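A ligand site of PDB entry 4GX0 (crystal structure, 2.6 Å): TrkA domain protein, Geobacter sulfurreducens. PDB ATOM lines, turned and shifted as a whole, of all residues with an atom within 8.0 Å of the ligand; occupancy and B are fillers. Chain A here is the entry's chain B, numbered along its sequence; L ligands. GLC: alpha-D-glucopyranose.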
ATOM      1  N   PRO A 227      21.157  24.741  23.324  1.00  0.00           N
ATOM      2  CA  PRO A 227      20.341  24.188  22.227  1.00  0.00           C
ATOM      3  C   PRO A 227      19.132  25.039  21.845  1.00  0.00           C
ATOM      4  O   PRO A 227      18.711  25.002  20.690  1.00  0.00           O
ATOM      5  CB  PRO A 227      19.901  22.849  22.779  1.00  0.00           C
ATOM      6  CG  PRO A 227      21.045  22.416  23.628  1.00  0.00           C
ATOM      7  CD  PRO A 227      21.598  23.687  24.248  1.00  0.00           C
ATOM      8  N   PRO A 243      25.192  22.023  18.422  1.00  0.00           N
ATOM      9  CA  PRO A 243      25.004  22.041  19.882  1.00  0.00           C
ATOM     10  C   PRO A 243      25.915  21.036  20.575  1.00  0.00           C
ATOM     11  O   PRO A 243      25.467  19.962  20.962  1.00  0.00           O
ATOM     12  CB  PRO A 243      23.541  21.608  20.035  1.00  0.00           C
ATOM     13  CG  PRO A 243      23.289  20.725  18.856  1.00  0.00           C
ATOM     14  CD  PRO A 243      24.123  21.290  17.728  1.00  0.00           C
ATOM     15  N   ARG A 246      24.989  19.518  24.075  1.00  0.00           N
ATOM     16  CA  ARG A 246      23.848  18.631  23.950  1.00  0.00           C
ATOM     17  C   ARG A 246      24.309  17.287  23.390  1.00  0.00           C
ATOM     18  O   ARG A 246      23.987  16.227  23.930  1.00  0.00           O
ATOM     19  CB  ARG A 246      22.788  19.233  23.025  1.00  0.00           C
ATOM     20  CG  ARG A 246      21.479  18.463  22.995  1.00  0.00           C
ATOM     21  CD  ARG A 246      20.573  18.992  21.896  1.00  0.00           C
ATOM     22  NE  ARG A 246      19.211  18.486  22.011  1.00  0.00           N
ATOM     23  CZ  ARG A 246      18.121  19.250  21.921  1.00  0.00           C
ATOM     24  NH1 ARG A 246      18.247  20.554  21.709  1.00  0.00           N
ATOM     25  NH2 ARG A 246      16.921  18.713  22.050  1.00  0.00           N
ATOM     26  N   ILE A 247      25.062  17.348  22.297  1.00  0.00           N
ATOM     27  CA  ILE A 247      25.621  16.169  21.662  1.00  0.00           C
ATOM     28  C   ILE A 247      26.522  15.379  22.620  1.00  0.00           C
ATOM     29  O   ILE A 247      26.455  14.157  22.694  1.00  0.00           O
ATOM     30  CB  ILE A 247      26.442  16.558  20.425  1.00  0.00           C
ATOM     31  CG1 ILE A 247      25.538  17.215  19.385  1.00  0.00           C
ATOM     32  CG2 ILE A 247      27.168  15.339  19.860  1.00  0.00           C
ATOM     33  CD1 ILE A 247      26.275  17.746  18.177  1.00  0.00           C
ATOM     34  N   ARG A 250      24.619  13.585  25.249  1.00  0.00           N
ATOM     35  CA  ARG A 250      23.972  12.425  24.650  1.00  0.00           C
ATOM     36  C   ARG A 250      24.929  11.238  24.525  1.00  0.00           C
ATOM     37  O   ARG A 250      24.572  10.106  24.829  1.00  0.00           O
ATOM     38  CB  ARG A 250      23.413  12.791  23.271  1.00  0.00           C
ATOM     39  CG  ARG A 250      22.747  11.642  22.539  1.00  0.00           C
ATOM     40  CD  ARG A 250      22.006  12.128  21.308  1.00  0.00           C
ATOM     41  NE  ARG A 250      21.619  11.019  20.439  1.00  0.00           N
ATOM     42  CZ  ARG A 250      22.446  10.443  19.568  1.00  0.00           C
ATOM     43  NH1 ARG A 250      22.030   9.438  18.814  1.00  0.00           N
ATOM     44  NH2 ARG A 250      23.692  10.879  19.458  1.00  0.00           N
ATOM     45  N   TYR A 251      26.158  11.508  24.088  1.00  0.00           N
ATOM     46  CA  TYR A 251      27.139  10.450  23.929  1.00  0.00           C
ATOM     47  C   TYR A 251      27.593   9.859  25.265  1.00  0.00           C
ATOM     48  O   TYR A 251      28.021   8.708  25.328  1.00  0.00           O
ATOM     49  CB  TYR A 251      28.335  10.934  23.109  1.00  0.00           C
ATOM     50  CG  TYR A 251      28.091  10.929  21.612  1.00  0.00           C
ATOM     51  CD1 TYR A 251      27.467   9.853  21.001  1.00  0.00           C
ATOM     52  CD2 TYR A 251      28.484  11.999  20.820  1.00  0.00           C
ATOM     53  CE1 TYR A 251      27.234   9.836  19.643  1.00  0.00           C
ATOM     54  CE2 TYR A 251      28.257  11.998  19.457  1.00  0.00           C
ATOM     55  CZ  TYR A 251      27.630  10.913  18.874  1.00  0.00           C
ATOM     56  OH  TYR A 251      27.408  10.905  17.516  1.00  0.00           O
ATOM     57  N   ALA A 263      19.556   4.854  19.488  1.00  0.00           N
ATOM     58  CA  ALA A 263      19.473   6.305  19.643  1.00  0.00           C
ATOM     59  C   ALA A 263      19.331   6.965  18.282  1.00  0.00           C
ATOM     60  O   ALA A 263      20.210   6.836  17.424  1.00  0.00           O
ATOM     61  CB  ALA A 263      20.701   6.833  20.382  1.00  0.00           C
ATOM     62  N   HIS A 264      18.229   7.676  18.085  1.00  0.00           N
ATOM     63  CA  HIS A 264      17.927   8.290  16.799  1.00  0.00           C
ATOM     64  C   HIS A 264      18.868   9.453  16.478  1.00  0.00           C
ATOM     65  O   HIS A 264      19.250  10.222  17.364  1.00  0.00           O
ATOM     66  CB  HIS A 264      16.475   8.766  16.773  1.00  0.00           C
ATOM     67  CG  HIS A 264      15.963   9.097  15.399  1.00  0.00           C
ATOM     68  ND1 HIS A 264      15.729   8.119  14.453  1.00  0.00           N
ATOM     69  CD2 HIS A 264      15.636  10.276  14.825  1.00  0.00           C
ATOM     70  CE1 HIS A 264      15.285   8.694  13.342  1.00  0.00           C
ATOM     71  NE2 HIS A 264      15.225  10.002  13.542  1.00  0.00           N
ATOM     72  N   ILE A 265      19.243   9.573  15.207  1.00  0.00           N
ATOM     73  CA  ILE A 265      20.154  10.615  14.753  1.00  0.00           C
ATOM     74  C   ILE A 265      19.514  11.560  13.738  1.00  0.00           C
ATOM     75  O   ILE A 265      19.528  12.782  13.912  1.00  0.00           O
ATOM     76  CB  ILE A 265      21.434  10.019  14.126  1.00  0.00           C
ATOM     77  CG1 ILE A 265      22.338   9.425  15.205  1.00  0.00           C
ATOM     78  CG2 ILE A 265      22.199  11.073  13.334  1.00  0.00           C
ATOM     79  CD1 ILE A 265      23.650   8.895  14.664  1.00  0.00           C
ATOM     80  N   LEU A 266      18.944  10.996  12.674  1.00  0.00           N
ATOM     81  CA  LEU A 266      18.372  11.798  11.607  1.00  0.00           C
ATOM     82  C   LEU A 266      17.092  11.189  11.020  1.00  0.00           C
ATOM     83  O   LEU A 266      16.984   9.977  10.890  1.00  0.00           O
ATOM     84  CB  LEU A 266      19.390  11.986  10.474  1.00  0.00           C
ATOM     85  CG  LEU A 266      18.844  12.511   9.144  1.00  0.00           C
ATOM     86  CD1 LEU A 266      18.460  13.983   9.260  1.00  0.00           C
ATOM     87  CD2 LEU A 266      19.854  12.310   8.007  1.00  0.00           C
ATOM     88  N   ASP A 267      16.142  12.048  10.677  1.00  0.00           N
ATOM     89  CA  ASP A 267      14.946  11.625   9.962  1.00  0.00           C
ATOM     90  C   ASP A 267      14.866  12.331   8.615  1.00  0.00           C
ATOM     91  O   ASP A 267      14.541  13.515   8.533  1.00  0.00           O
ATOM     92  CB  ASP A 267      13.688  11.913  10.798  1.00  0.00           C
ATOM     93  CG  ASP A 267      12.417  11.491  10.081  1.00  0.00           C
ATOM     94  OD1 ASP A 267      12.509  10.699   9.128  1.00  0.00           O
ATOM     95  OD2 ASP A 267      11.326  11.944  10.490  1.00  0.00           O
ATOM     96  N   ILE A 274      18.283   7.329  10.429  1.00  0.00           N
ATOM     97  CA  ILE A 274      19.647   7.019  10.860  1.00  0.00           C
ATOM     98  C   ILE A 274      19.699   6.974  12.385  1.00  0.00           C
ATOM     99  O   ILE A 274      19.276   7.910  13.057  1.00  0.00           O
ATOM    100  CB  ILE A 274      20.652   8.051  10.343  1.00  0.00           C
ATOM    101  CG1 ILE A 274      20.616   8.120   8.813  1.00  0.00           C
ATOM    102  CG2 ILE A 274      22.057   7.710  10.825  1.00  0.00           C
ATOM    103  CD1 ILE A 274      21.593   9.115   8.225  1.00  0.00           C
ATOM    104  N   GLU A 276      22.038   5.196  16.007  1.00  0.00           N
ATOM    105  CA  GLU A 276      23.252   4.542  16.475  1.00  0.00           C
ATOM    106  C   GLU A 276      22.991   3.647  17.678  1.00  0.00           C
ATOM    107  O   GLU A 276      22.106   3.922  18.480  1.00  0.00           O
ATOM    108  CB  GLU A 276      24.372   5.555  16.751  1.00  0.00           C
ATOM    109  CG  GLU A 276      23.946   6.748  17.587  1.00  0.00           C
ATOM    110  CD  GLU A 276      25.014   7.827  17.646  1.00  0.00           C
ATOM    111  OE1 GLU A 276      26.204   7.497  17.437  1.00  0.00           O
ATOM    112  OE2 GLU A 276      24.662   8.998  17.880  1.00  0.00           O
ATOM    113  N   ALA A 362      22.951  18.085  29.987  1.00  0.00           N
ATOM    114  CA  ALA A 362      22.466  17.510  28.740  1.00  0.00           C
ATOM    115  C   ALA A 362      22.343  15.990  28.820  1.00  0.00           C
ATOM    116  O   ALA A 362      21.440  15.403  28.235  1.00  0.00           O
ATOM    117  CB  ALA A 362      23.379  17.904  27.586  1.00  0.00           C
ATOM    118  N   ALA A 365      19.105  15.359  30.577  1.00  0.00           N
ATOM    119  CA  ALA A 365      17.976  15.610  29.696  1.00  0.00           C
ATOM    120  C   ALA A 365      17.779  14.445  28.729  1.00  0.00           C
ATOM    121  O   ALA A 365      16.649  14.018  28.472  1.00  0.00           O
ATOM    122  CB  ALA A 365      18.159  16.907  28.935  1.00  0.00           C
ATOM    123  N   PHE A 366      18.880  13.936  28.191  1.00  0.00           N
ATOM    124  CA  PHE A 366      18.816  12.784  27.297  1.00  0.00           C
ATOM    125  C   PHE A 366      18.239  11.565  27.991  1.00  0.00           C
ATOM    126  O   PHE A 366      17.352  10.899  27.460  1.00  0.00           O
ATOM    127  CB  PHE A 366      20.187  12.437  26.737  1.00  0.00           C
ATOM    128  CG  PHE A 366      20.216  11.128  26.004  1.00  0.00           C
ATOM    129  CD1 PHE A 366      19.907  11.068  24.666  1.00  0.00           C
ATOM    130  CD2 PHE A 366      20.545   9.952  26.672  1.00  0.00           C
ATOM    131  CE1 PHE A 366      19.921   9.861  23.995  1.00  0.00           C
ATOM    132  CE2 PHE A 366      20.561   8.752  26.008  1.00  0.00           C
ATOM    133  CZ  PHE A 366      20.250   8.706  24.670  1.00  0.00           C
ATOM    134  N   ARG A 369      14.610  11.614  28.424  1.00  0.00           N
ATOM    135  CA  ARG A 369      13.856  11.473  27.183  1.00  0.00           C
ATOM    136  C   ARG A 369      13.381  10.044  26.972  1.00  0.00           C
ATOM    137  O   ARG A 369      12.595   9.773  26.058  1.00  0.00           O
ATOM    138  CB  ARG A 369      14.712  11.916  25.996  1.00  0.00           C
ATOM    139  CG  ARG A 369      13.999  12.806  24.983  1.00  0.00           C
ATOM    140  CD  ARG A 369      14.548  14.234  25.033  1.00  0.00           C
ATOM    141  NE  ARG A 369      15.979  14.292  24.791  1.00  0.00           N
ATOM    142  CZ  ARG A 369      16.700  15.410  24.747  1.00  0.00           C
ATOM    143  NH1 ARG A 369      18.002  15.366  24.520  1.00  0.00           N
ATOM    144  NH2 ARG A 369      16.103  16.591  24.931  1.00  0.00           N
HETATM  145  C1  GLC L   1      16.533  15.849  18.447  1.00  0.00           C
HETATM  146  C2  GLC L   1      16.563  15.602  19.932  1.00  0.00           C
HETATM  147  C3  GLC L   1      17.897  15.520  20.444  1.00  0.00           C
HETATM  148  C4  GLC L   1      18.701  14.595  19.722  1.00  0.00           C
HETATM  149  C5  GLC L   1      18.663  14.841  18.243  1.00  0.00           C
HETATM  150  C6  GLC L   1      19.374  13.787  17.472  1.00  0.00           C
HETATM  151  O1  GLC L   1      16.971  17.120  18.105  1.00  0.00           O
HETATM  152  O2  GLC L   1      15.929  16.661  20.566  1.00  0.00           O
HETATM  153  O3  GLC L   1      17.805  15.002  21.739  1.00  0.00           O
HETATM  154  O4  GLC L   1      20.075  14.762  20.115  1.00  0.00           O
HETATM  155  O5  GLC L   1      17.299  14.924  17.742  1.00  0.00           O
HETATM  156  O6  GLC L   1      20.672  13.998  17.154  1.00  0.00           O
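O3 of the ligand is in hydrogen-bond range of NH1 of Arg 369 (2.8 Å).
The guanidinium group of Arg 246 lies within hydrogen-bond range of an oxygen (O2) of the ligand (2.7 Å).
Arg 250 touches the ligand.
His 264 touches the ligand (O to C6, 3.6 Å).
Ile 265 touches the ligand (O to O6, 3.6 Å).
Within 4 Å of the ligand: Arg 246, Arg 250, His 264, Ile 265 and Arg 369.
The backbone carbonyl oxygen (O) of Ala 263 lies close to the guanidinium group (NH1) of Arg 250 (3.5 Å).
NH1 of Arg 250 is in hydrogen-bond range of O of His 264, 3.2 Å away.
NE2 of His 264 is in hydrogen-bond range of O of Leu 266 (3.2 Å).
The backbone NH of Ile 265 sits at hydrogen-bond distance from the backbone carbonyl oxygen of Ile 274, at 2.7 Å.
The side-chain carboxylate of Glu 276 is in salt-bridge range of the guanidinium group of Arg 250 (2.6 Å).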
